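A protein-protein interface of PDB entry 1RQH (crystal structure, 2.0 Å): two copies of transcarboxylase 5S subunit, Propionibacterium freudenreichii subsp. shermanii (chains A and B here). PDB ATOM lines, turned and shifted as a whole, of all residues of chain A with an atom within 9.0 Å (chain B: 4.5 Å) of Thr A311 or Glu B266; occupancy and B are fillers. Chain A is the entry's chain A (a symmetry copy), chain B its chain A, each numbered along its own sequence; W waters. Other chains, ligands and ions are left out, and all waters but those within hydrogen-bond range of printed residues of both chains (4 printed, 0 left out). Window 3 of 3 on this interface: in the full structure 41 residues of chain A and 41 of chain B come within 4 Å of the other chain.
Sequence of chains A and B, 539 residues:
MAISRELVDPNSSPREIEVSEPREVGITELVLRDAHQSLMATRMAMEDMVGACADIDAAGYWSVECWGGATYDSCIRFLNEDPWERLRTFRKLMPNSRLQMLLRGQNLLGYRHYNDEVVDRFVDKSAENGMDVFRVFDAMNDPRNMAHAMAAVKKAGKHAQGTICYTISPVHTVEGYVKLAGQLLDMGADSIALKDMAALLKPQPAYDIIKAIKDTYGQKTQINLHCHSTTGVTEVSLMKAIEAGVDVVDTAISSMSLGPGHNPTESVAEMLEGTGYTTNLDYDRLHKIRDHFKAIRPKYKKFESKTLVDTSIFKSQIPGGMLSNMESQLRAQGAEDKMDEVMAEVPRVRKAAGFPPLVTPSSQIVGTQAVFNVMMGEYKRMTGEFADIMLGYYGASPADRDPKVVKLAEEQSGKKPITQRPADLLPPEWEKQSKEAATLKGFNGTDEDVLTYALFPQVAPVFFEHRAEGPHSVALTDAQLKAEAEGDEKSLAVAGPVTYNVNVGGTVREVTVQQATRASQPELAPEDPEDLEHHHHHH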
ATOM      1  N   ALA A 198      14.249  15.099 -22.098  1.00  0.00           N
ATOM      2  CA  ALA A 198      13.063  15.860 -22.476  1.00  0.00           C
ATOM      3  C   ALA A 198      12.649  16.791 -21.331  1.00  0.00           C
ATOM      4  O   ALA A 198      11.573  17.388 -21.379  1.00  0.00           O
ATOM      5  CB  ALA A 198      11.916  14.901 -22.827  1.00  0.00           C
ATOM      6  N   ALA A 199      13.501  16.917 -20.313  1.00  0.00           N
ATOM      7  CA  ALA A 199      13.220  17.777 -19.152  1.00  0.00           C
ATOM      8  C   ALA A 199      11.943  17.311 -18.446  1.00  0.00           C
ATOM      9  O   ALA A 199      11.126  18.128 -18.000  1.00  0.00           O
ATOM     10  CB  ALA A 199      13.078  19.250 -19.591  1.00  0.00           C
ATOM     11  N   LEU A 200      11.786  15.999 -18.313  1.00  0.00           N
ATOM     12  CA  LEU A 200      10.597  15.431 -17.682  1.00  0.00           C
ATOM     13  C   LEU A 200      10.791  15.250 -16.181  1.00  0.00           C
ATOM     14  O   LEU A 200       9.814  15.017 -15.465  1.00  0.00           O
ATOM     15  CB  LEU A 200      10.312  14.063 -18.294  1.00  0.00           C
ATOM     16  CG  LEU A 200       9.632  13.997 -19.655  1.00  0.00           C
ATOM     17  CD1 LEU A 200       9.781  12.592 -20.234  1.00  0.00           C
ATOM     18  CD2 LEU A 200       8.168  14.376 -19.486  1.00  0.00           C
ATOM     19  N   LYS A 202      10.826  16.061 -12.591  1.00  0.00           N
ATOM     20  CA  LYS A 202      10.327  17.093 -11.693  1.00  0.00           C
ATOM     21  C   LYS A 202      11.122  17.030 -10.389  1.00  0.00           C
ATOM     22  O   LYS A 202      11.829  16.063 -10.124  1.00  0.00           O
ATOM     23  CB  LYS A 202       8.815  16.912 -11.439  1.00  0.00           C
ATOM     24  CG  LYS A 202       8.064  17.198 -12.576  1.00  0.00           C
ATOM     25  CD  LYS A 202       6.698  17.172 -12.302  1.00  0.00           C
ATOM     26  CE  LYS A 202       5.919  17.542 -13.393  1.00  0.00           C
ATOM     27  NZ  LYS A 202       4.451  17.786 -13.074  1.00  0.00           N
ATOM     28  N   SER A 229      16.340  21.955 -20.113  1.00  0.00           N
ATOM     29  CA  SER A 229      15.475  22.963 -19.484  1.00  0.00           C
ATOM     30  C   SER A 229      14.207  23.201 -20.301  1.00  0.00           C
ATOM     31  O   SER A 229      13.475  24.158 -20.052  1.00  0.00           O
ATOM     32  CB  SER A 229      16.252  24.269 -19.390  1.00  0.00           C
ATOM     33  OG  SER A 229      16.826  24.578 -20.656  1.00  0.00           O
ATOM     34  N   THR A 230      13.947  22.320 -21.255  1.00  0.00           N
ATOM     35  CA  THR A 230      12.812  22.416 -22.176  1.00  0.00           C
ATOM     36  C   THR A 230      11.480  22.764 -21.484  1.00  0.00           C
ATOM     37  O   THR A 230      10.756  23.630 -21.973  1.00  0.00           O
ATOM     38  CB  THR A 230      12.642  21.098 -22.934  1.00  0.00           C
ATOM     39  OG1 THR A 230      13.935  20.637 -23.353  1.00  0.00           O
ATOM     40  CG2 THR A 230      11.749  21.305 -24.167  1.00  0.00           C
ATOM     41  N   THR A 231      11.148  22.099 -20.376  1.00  0.00           N
ATOM     42  CA  THR A 231       9.872  22.316 -19.678  1.00  0.00           C
ATOM     43  C   THR A 231       9.982  23.425 -18.630  1.00  0.00           C
ATOM     44  O   THR A 231       8.969  23.817 -18.044  1.00  0.00           O
ATOM     45  CB  THR A 231       9.415  21.053 -18.937  1.00  0.00           C
ATOM     46  OG1 THR A 231      10.421  20.689 -17.982  1.00  0.00           O
ATOM     47  CG2 THR A 231       9.184  19.904 -19.912  1.00  0.00           C
ATOM     48  N   GLY A 232      11.192  23.900 -18.363  1.00  0.00           N
ATOM     49  CA  GLY A 232      11.376  24.966 -17.394  1.00  0.00           C
ATOM     50  C   GLY A 232      11.299  24.629 -15.912  1.00  0.00           C
ATOM     51  O   GLY A 232      11.286  25.545 -15.095  1.00  0.00           O
ATOM     52  N   VAL A 233      11.295  23.346 -15.544  1.00  0.00           N
ATOM     53  CA  VAL A 233      11.173  22.978 -14.126  1.00  0.00           C
ATOM     54  C   VAL A 233      12.453  22.312 -13.592  1.00  0.00           C
ATOM     55  O   VAL A 233      12.559  22.081 -12.382  1.00  0.00           O
ATOM     56  CB  VAL A 233      10.047  21.910 -13.887  1.00  0.00           C
ATOM     57  CG1 VAL A 233       8.770  22.258 -14.650  1.00  0.00           C
ATOM     58  CG2 VAL A 233      10.538  20.529 -14.328  1.00  0.00           C
ATOM     59  N   THR A 234      13.427  22.037 -14.451  1.00  0.00           N
ATOM     60  CA  THR A 234      14.574  21.233 -14.015  1.00  0.00           C
ATOM     61  C   THR A 234      15.630  21.953 -13.188  1.00  0.00           C
ATOM     62  O   THR A 234      16.419  21.259 -12.543  1.00  0.00           O
ATOM     63  CB  THR A 234      15.234  20.501 -15.193  1.00  0.00           C
ATOM     64  OG1 THR A 234      15.708  21.448 -16.155  1.00  0.00           O
ATOM     65  CG2 THR A 234      14.218  19.551 -15.834  1.00  0.00           C
ATOM     66  N   THR A 307      11.071  28.181 -29.199  1.00  0.00           N
ATOM     67  CA  THR A 307      10.263  28.028 -27.979  1.00  0.00           C
ATOM     68  C   THR A 307      11.179  27.859 -26.771  1.00  0.00           C
ATOM     69  O   THR A 307      11.956  26.909 -26.707  1.00  0.00           O
ATOM     70  CB  THR A 307       9.310  26.812 -28.066  1.00  0.00           C
ATOM     71  OG1 THR A 307       8.514  26.908 -29.257  1.00  0.00           O
ATOM     72  CG2 THR A 307       8.376  26.777 -26.845  1.00  0.00           C
ATOM     73  N   LEU A 308      11.075  28.776 -25.810  1.00  0.00           N
ATOM     74  CA  LEU A 308      11.915  28.744 -24.612  1.00  0.00           C
ATOM     75  C   LEU A 308      11.353  27.795 -23.551  1.00  0.00           C
ATOM     76  O   LEU A 308      12.115  27.166 -22.825  1.00  0.00           O
ATOM     77  CB  LEU A 308      12.026  30.147 -24.013  1.00  0.00           C
ATOM     78  CG  LEU A 308      13.028  31.125 -24.622  1.00  0.00           C
ATOM     79  CD1 LEU A 308      13.119  32.344 -23.722  1.00  0.00           C
ATOM     80  CD2 LEU A 308      14.401  30.461 -24.753  1.00  0.00           C
ATOM     81  N   VAL A 309      10.033  27.700 -23.438  1.00  0.00           N
ATOM     82  CA  VAL A 309       9.440  26.838 -22.415  1.00  0.00           C
ATOM     83  C   VAL A 309       8.219  26.133 -22.978  1.00  0.00           C
ATOM     84  O   VAL A 309       7.356  26.769 -23.583  1.00  0.00           O
ATOM     85  CB  VAL A 309       8.989  27.665 -21.169  1.00  0.00           C
ATOM     86  CG1 VAL A 309       8.422  26.737 -20.092  1.00  0.00           C
ATOM     87  CG2 VAL A 309      10.154  28.442 -20.610  1.00  0.00           C
ATOM     88  N   ASP A 310       8.147  24.820 -22.769  1.00  0.00           N
ATOM     89  CA  ASP A 310       7.011  24.031 -23.240  1.00  0.00           C
ATOM     90  C   ASP A 310       6.765  22.889 -22.259  1.00  0.00           C
ATOM     91  O   ASP A 310       7.558  21.962 -22.175  1.00  0.00           O
ATOM     92  CB  ASP A 310       7.313  23.481 -24.633  1.00  0.00           C
ATOM     93  CG  ASP A 310       6.129  22.759 -25.237  1.00  0.00           C
ATOM     94  OD1 ASP A 310       5.075  22.681 -24.568  1.00  0.00           O
ATOM     95  OD2 ASP A 310       6.257  22.269 -26.381  1.00  0.00           O
ATOM     96  N   THR A 311       5.655  22.965 -21.528  1.00  0.00           N
ATOM     97  CA  THR A 311       5.306  21.969 -20.514  1.00  0.00           C
ATOM     98  C   THR A 311       4.261  20.980 -21.055  1.00  0.00           C
ATOM     99  O   THR A 311       3.808  20.097 -20.322  1.00  0.00           O
ATOM    100  CB  THR A 311       4.665  22.650 -19.290  1.00  0.00           C
ATOM    101  OG1 THR A 311       3.519  23.387 -19.729  1.00  0.00           O
ATOM    102  CG2 THR A 311       5.635  23.625 -18.610  1.00  0.00           C
ATOM    103  N   SER A 312       3.878  21.113 -22.321  1.00  0.00           N
ATOM    104  CA  SER A 312       2.835  20.263 -22.890  1.00  0.00           C
ATOM    105  C   SER A 312       3.175  18.769 -22.768  1.00  0.00           C
ATOM    106  O   SER A 312       2.269  17.940 -22.655  1.00  0.00           O
ATOM    107  CB  SER A 312       2.600  20.652 -24.358  1.00  0.00           C
ATOM    108  OG  SER A 312       3.771  20.483 -25.133  1.00  0.00           O
ATOM    109  N   ILE A 313       4.456  18.417 -22.760  1.00  0.00           N
ATOM    110  CA  ILE A 313       4.854  17.009 -22.689  1.00  0.00           C
ATOM    111  C   ILE A 313       4.367  16.342 -21.388  1.00  0.00           C
ATOM    112  O   ILE A 313       4.194  15.126 -21.348  1.00  0.00           O
ATOM    113  CB  ILE A 313       6.383  16.849 -22.795  1.00  0.00           C
ATOM    114  CG1 ILE A 313       6.733  15.376 -23.033  1.00  0.00           C
ATOM    115  CG2 ILE A 313       7.057  17.349 -21.520  1.00  0.00           C
ATOM    116  CD1 ILE A 313       8.230  15.105 -23.199  1.00  0.00           C
ATOM    117  N   PHE A 314       4.162  17.113 -20.326  1.00  0.00           N
ATOM    118  CA  PHE A 314       3.710  16.524 -19.067  1.00  0.00           C
ATOM    119  C   PHE A 314       2.311  15.942 -19.233  1.00  0.00           C
ATOM    120  O   PHE A 314       1.871  15.126 -18.428  1.00  0.00           O
ATOM    121  CB  PHE A 314       3.724  17.587 -17.965  1.00  0.00           C
ATOM    122  CG  PHE A 314       5.106  17.938 -17.486  1.00  0.00           C
ATOM    123  CD1 PHE A 314       5.510  19.267 -17.389  1.00  0.00           C
ATOM    124  CD2 PHE A 314       5.998  16.939 -17.112  1.00  0.00           C
ATOM    125  CE1 PHE A 314       6.790  19.590 -16.923  1.00  0.00           C
ATOM    126  CE2 PHE A 314       7.274  17.250 -16.646  1.00  0.00           C
ATOM    127  CZ  PHE A 314       7.671  18.576 -16.550  1.00  0.00           C
ATOM    128  N   LYS A 315       1.616  16.362 -20.278  1.00  0.00           N
ATOM    129  CA  LYS A 315       0.271  15.864 -20.534  1.00  0.00           C
ATOM    130  C   LYS A 315       0.260  14.907 -21.731  1.00  0.00           C
ATOM    131  O   LYS A 315      -0.425  13.891 -21.696  1.00  0.00           O
ATOM    132  CB  LYS A 315      -0.674  17.029 -20.845  1.00  0.00           C
ATOM    133  CG  LYS A 315      -1.914  16.545 -21.248  1.00  0.00           C
ATOM    134  CD  LYS A 315      -2.789  17.543 -21.664  1.00  0.00           C
ATOM    135  CE  LYS A 315      -3.994  16.991 -22.084  1.00  0.00           C
ATOM    136  NZ  LYS A 315      -4.993  18.008 -22.527  1.00  0.00           N
ATOM    137  N   SER A 316       1.031  15.215 -22.768  1.00  0.00           N
ATOM    138  CA  SER A 316       0.999  14.430 -24.004  1.00  0.00           C
ATOM    139  C   SER A 316       2.064  13.323 -24.074  1.00  0.00           C
ATOM    140  O   SER A 316       1.910  12.404 -24.882  1.00  0.00           O
ATOM    141  CB  SER A 316       1.205  15.364 -25.184  1.00  0.00           C
ATOM    142  OG  SER A 316       2.552  15.816 -25.208  1.00  0.00           O
ATOM    143  N   GLN A 317       3.122  13.392 -23.273  1.00  0.00           N
ATOM    144  CA  GLN A 317       4.198  12.391 -23.351  1.00  0.00           C
ATOM    145  C   GLN A 317       4.973  12.568 -24.658  1.00  0.00           C
ATOM    146  O   GLN A 317       5.884  11.793 -24.942  1.00  0.00           O
ATOM    147  CB  GLN A 317       3.647  10.964 -23.381  1.00  0.00           C
ATOM    148  CG  GLN A 317       3.010  10.583 -22.207  1.00  0.00           C
ATOM    149  CD  GLN A 317       2.518   9.144 -22.324  1.00  0.00           C
ATOM    150  OE1 GLN A 317       3.291   8.229 -22.647  1.00  0.00           O
ATOM    151  NE2 GLN A 317       1.231   8.938 -22.080  1.00  0.00           N
ATOM    152  N   ILE A 318       4.626  13.571 -25.457  1.00  0.00           N
ATOM    153  CA  ILE A 318       5.298  13.745 -26.741  1.00  0.00           C
ATOM    154  C   ILE A 318       6.283  14.904 -26.703  1.00  0.00           C
ATOM    155  O   ILE A 318       5.907  16.048 -26.452  1.00  0.00           O
ATOM    156  CB  ILE A 318       4.289  14.016 -27.874  1.00  0.00           C
ATOM    157  CG1 ILE A 318       3.281  12.874 -27.965  1.00  0.00           C
ATOM    158  CG2 ILE A 318       5.029  14.168 -29.193  1.00  0.00           C
ATOM    159  CD1 ILE A 318       2.196  13.093 -29.010  1.00  0.00           C
ATOM    160  N   GLY A 320       8.632  17.833 -27.999  1.00  0.00           N
ATOM    161  CA  GLY A 320       8.452  18.783 -29.085  1.00  0.00           C
ATOM    162  C   GLY A 320       9.062  18.344 -30.405  1.00  0.00           C
ATOM    163  O   GLY A 320       8.439  18.473 -31.460  1.00  0.00           O
ATOM    164  N   ILE B 253       2.782  33.662 -18.081  1.00  0.00           N
ATOM    165  CA  ILE B 253       2.486  32.530 -18.965  1.00  0.00           C
ATOM    166  C   ILE B 253       3.767  32.199 -19.756  1.00  0.00           C
ATOM    167  O   ILE B 253       4.485  33.108 -20.187  1.00  0.00           O
ATOM    168  CB  ILE B 253       1.264  32.865 -19.889  1.00  0.00           C
ATOM    169  CG1 ILE B 253       0.595  31.569 -20.381  1.00  0.00           C
ATOM    170  CG2 ILE B 253       1.705  33.741 -21.051  1.00  0.00           C
ATOM    171  CD1 ILE B 253      -0.114  30.785 -19.282  1.00  0.00           C
ATOM    172  N   SER B 254       4.040  30.906 -19.944  1.00  0.00           N
ATOM    173  CA  SER B 254       5.273  30.385 -20.569  1.00  0.00           C
ATOM    174  C   SER B 254       5.686  31.061 -21.895  1.00  0.00           C
ATOM    175  O   SER B 254       6.886  31.244 -22.115  1.00  0.00           O
ATOM    176  CB  SER B 254       5.143  28.866 -20.778  1.00  0.00           C
ATOM    177  OG  SER B 254       4.100  28.562 -21.685  1.00  0.00           O
ATOM    178  N   PRO B 264       8.085  30.998 -15.615  1.00  0.00           N
ATOM    179  CA  PRO B 264       6.848  30.542 -16.257  1.00  0.00           C
ATOM    180  C   PRO B 264       5.746  29.996 -15.369  1.00  0.00           C
ATOM    181  O   PRO B 264       5.967  29.125 -14.531  1.00  0.00           O
ATOM    182  CB  PRO B 264       7.342  29.501 -17.272  1.00  0.00           C
ATOM    183  CG  PRO B 264       8.856  29.645 -17.274  1.00  0.00           C
ATOM    184  CD  PRO B 264       9.161  30.028 -15.867  1.00  0.00           C
ATOM    185  N   THR B 265       4.538  30.495 -15.605  1.00  0.00           N
ATOM    186  CA  THR B 265       3.365  30.088 -14.838  1.00  0.00           C
ATOM    187  C   THR B 265       3.213  28.567 -14.845  1.00  0.00           C
ATOM    188  O   THR B 265       3.145  27.954 -13.780  1.00  0.00           O
ATOM    189  CB  THR B 265       2.094  30.735 -15.420  1.00  0.00           C
ATOM    190  OG1 THR B 265       2.231  32.160 -15.355  1.00  0.00           O
ATOM    191  CG2 THR B 265       0.833  30.288 -14.650  1.00  0.00           C
ATOM    192  N   GLU B 266       3.177  27.963 -16.035  1.00  0.00           N
ATOM    193  CA  GLU B 266       2.988  26.516 -16.159  1.00  0.00           C
ATOM    194  C   GLU B 266       4.133  25.734 -15.497  1.00  0.00           C
ATOM    195  O   GLU B 266       3.893  24.688 -14.883  1.00  0.00           O
ATOM    196  CB  GLU B 266       2.869  26.123 -17.642  1.00  0.00           C
ATOM    197  CG  GLU B 266       1.779  26.742 -18.245  1.00  0.00           C
ATOM    198  CD  GLU B 266       2.185  27.909 -19.136  1.00  0.00           C
ATOM    199  OE1 GLU B 266       2.742  28.896 -18.615  1.00  0.00           O
ATOM    200  OE2 GLU B 266       1.959  27.832 -20.360  1.00  0.00           O
ATOM    201  N   SER B 267       5.365  26.215 -15.640  1.00  0.00           N
ATOM    202  CA  SER B 267       6.529  25.539 -15.057  1.00  0.00           C
ATOM    203  C   SER B 267       6.424  25.538 -13.529  1.00  0.00           C
ATOM    204  O   SER B 267       6.640  24.515 -12.879  1.00  0.00           O
ATOM    205  CB  SER B 267       7.813  26.253 -15.498  1.00  0.00           C
ATOM    206  OG  SER B 267       7.967  26.209 -16.912  1.00  0.00           O
ATOM    207  N   VAL B 268       6.080  26.683 -12.948  1.00  0.00           N
ATOM    208  CA  VAL B 268       5.960  26.770 -11.496  1.00  0.00           C
ATOM    209  C   VAL B 268       4.830  25.864 -11.007  1.00  0.00           C
ATOM    210  O   VAL B 268       4.943  25.242  -9.949  1.00  0.00           O
ATOM    211  CB  VAL B 268       5.710  28.223 -11.054  1.00  0.00           C
ATOM    212  CG1 VAL B 268       5.216  28.263  -9.616  1.00  0.00           C
ATOM    213  CG2 VAL B 268       7.005  29.022 -11.203  1.00  0.00           C
ATOM    214  N   ALA B 269       3.744  25.775 -11.771  1.00  0.00           N
ATOM    215  CA  ALA B 269       2.624  24.921 -11.368  1.00  0.00           C
ATOM    216  C   ALA B 269       3.021  23.450 -11.476  1.00  0.00           C
ATOM    217  O   ALA B 269       2.734  22.656 -10.578  1.00  0.00           O
ATOM    218  CB  ALA B 269       1.398  25.187 -12.251  1.00  0.00           C
ATOM    219  N   GLU B 270       3.682  23.084 -12.574  1.00  0.00           N
ATOM    220  CA  GLU B 270       4.072  21.683 -12.801  1.00  0.00           C
ATOM    221  C   GLU B 270       5.159  21.212 -11.820  1.00  0.00           C
ATOM    222  O   GLU B 270       5.141  20.056 -11.407  1.00  0.00           O
ATOM    223  CB  GLU B 270       4.581  21.509 -14.240  1.00  0.00           C
ATOM    224  CG  GLU B 270       3.576  21.735 -15.174  1.00  0.00           C
ATOM    225  CD  GLU B 270       2.719  20.505 -15.469  1.00  0.00           C
ATOM    226  OE1 GLU B 270       2.798  19.499 -14.726  1.00  0.00           O
ATOM    227  OE2 GLU B 270       1.950  20.550 -16.454  1.00  0.00           O
ATOM    228  N   LEU B 286      -4.589  27.501 -19.170  1.00  0.00           N
ATOM    229  CA  LEU B 286      -3.220  28.005 -19.296  1.00  0.00           C
ATOM    230  C   LEU B 286      -2.698  27.752 -20.708  1.00  0.00           C
ATOM    231  O   LEU B 286      -2.026  28.599 -21.298  1.00  0.00           O
ATOM    232  CB  LEU B 286      -2.304  27.310 -18.281  1.00  0.00           C
ATOM    233  CG  LEU B 286      -2.550  27.542 -16.790  1.00  0.00           C
ATOM    234  CD1 LEU B 286      -1.424  26.886 -15.991  1.00  0.00           C
ATOM    235  CD2 LEU B 286      -2.611  29.038 -16.496  1.00  0.00           C
ATOM    236  N   ARG B 290      -1.275  30.503 -23.195  1.00  0.00           N
ATOM    237  CA  ARG B 290       0.054  30.350 -23.789  1.00  0.00           C
ATOM    238  C   ARG B 290      -0.042  30.657 -25.287  1.00  0.00           C
ATOM    239  O   ARG B 290       0.839  31.298 -25.865  1.00  0.00           O
ATOM    240  CB  ARG B 290       0.553  28.922 -23.555  1.00  0.00           C
ATOM    241  CG  ARG B 290       1.688  28.669 -24.316  1.00  0.00           C
ATOM    242  CD  ARG B 290       2.094  27.345 -24.186  1.00  0.00           C
ATOM    243  NE  ARG B 290       2.966  26.950 -25.292  1.00  0.00           N
ATOM    244  CZ  ARG B 290       4.279  27.150 -25.356  1.00  0.00           C
ATOM    245  NH1 ARG B 290       4.929  27.747 -24.363  1.00  0.00           N
ATOM    246  NH2 ARG B 290       4.940  26.770 -26.441  1.00  0.00           N
HETATM  247  O   HOH W   1       4.274  25.472 -21.864  1.00  0.00           O
HETATM  248  O   HOH W   2       1.551  22.907 -18.094  1.00  0.00           O
HETATM  249  O   HOH W   3       8.409  30.002 -24.251  1.00  0.00           O
HETATM  250  O   HOH W   4       1.267  19.652 -19.716  1.00  0.00           O
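The side-chain hydroxyl (OG) of Ser B267 sits at hydrogen-bond distance from the backbone carbonyl oxygen (O) of Thr A231, at 2.8 Å. The side-chain amino group (NZ) of Lys A202 is in salt-bridge range of the side-chain carboxylate (OE1) of Glu B270 (2.9 Å). O of Val A309 lies within hydrogen-bond range of NH1 of Arg B290.
The side-chain hydroxyl of Ser B254 lies within hydrogen-bond range of the side-chain carboxylate of Glu B266 (2.6 Å). The side-chain hydroxyl of Ser B254 sits at hydrogen-bond distance from the guanidinium group of Arg B290. The side-chain hydroxyl of Thr A231 is in hydrogen-bond range of the backbone carbonyl oxygen of Ala A199, 2.7 Å away.
Among the printed residues, pairs that only touch across the chains: Gly A232 with Ser B267 (3.6 Å), Val A233 with Ser B267 (3.6 Å), Thr A307 with Arg B290 (3.5 Å), Val A309 with Ser B254 (3.97 Å), Val A309 with Pro B264 (3.8 Å), Val A309 with Ser B267 (3.3 Å), Thr A311 with Glu B266 (3.5 Å), Thr A311 with Ser B267 (3.9 Å) and Phe A314 with Glu B270 (3.6 Å).
Printed residues of chain B within 4 Å of Gly A232: Ser B267. Of the printed residues of chain B, Val A309 touches Ser B254, Pro B264, Ser B267 and Arg B290. Of chain B, only Glu B266 (3.5 Å) and Ser B267 (3.9 Å) come within 4 Å of Thr A311. Ser A312 touches none of the printed residues of chain B. No residue of chain A comes within 4 Å of Thr B265. Glu B266 touches one residue of chain A. No residue of chain A comes within 4 Å of Ala B269. The nearest residue of chain B that does not touch Thr A311 is Glu B270 (4.3 Å).
Of the 11 printed residues of chain B, 6 touch a printed residue of chain A. Printed residues of chain A that touch a printed residue of chain B: Lys A202, Thr A231, Gly A232, Val A233, Thr A307, Val A309, Thr A311 and Phe A314. Hydrophobic or aromatic side chains of chain A within 4 Å of the printed part of chain B: Val A233, Val A309 and Phe A314. Among the printed residues, Asp or Glu carboxylates within 4 Å of a Lys or Arg side-chain nitrogen of the other chain: Lys A202 with Glu B270 (2.9 Å).
No position is printed for both chains. Of the 12 pairs that touch across the chains among the printed residues, none has its exchanged pair printed and touching as well.
Water W2 bridges the side-chain hydroxyl (OG1) of Thr A311 (2.6 Å) and the side-chain carboxylate (OE2) of Glu B270 (2.9 Å). Water W4 lies within hydrogen-bond range of O of Thr A311 (2.6 Å), N of Lys A315 (3.4 Å) and OE2 of Glu B270 (3.5 Å). Water W1 lies within hydrogen-bond range of the backbone NH (N) of Thr A311 (2.9 Å), the side-chain hydroxyl (OG) of Ser B254 (3.1 Å) and the guanidinium group (NH1) of Arg B290 (3.4 Å). Water W3 lies within hydrogen-bond range of the backbone carbonyl oxygen (O) of Ser B254 (2.9 Å), the backbone NH (N) of Val A309 (2.9 Å) and the backbone NH (N) of Leu A308 (3.3 Å).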
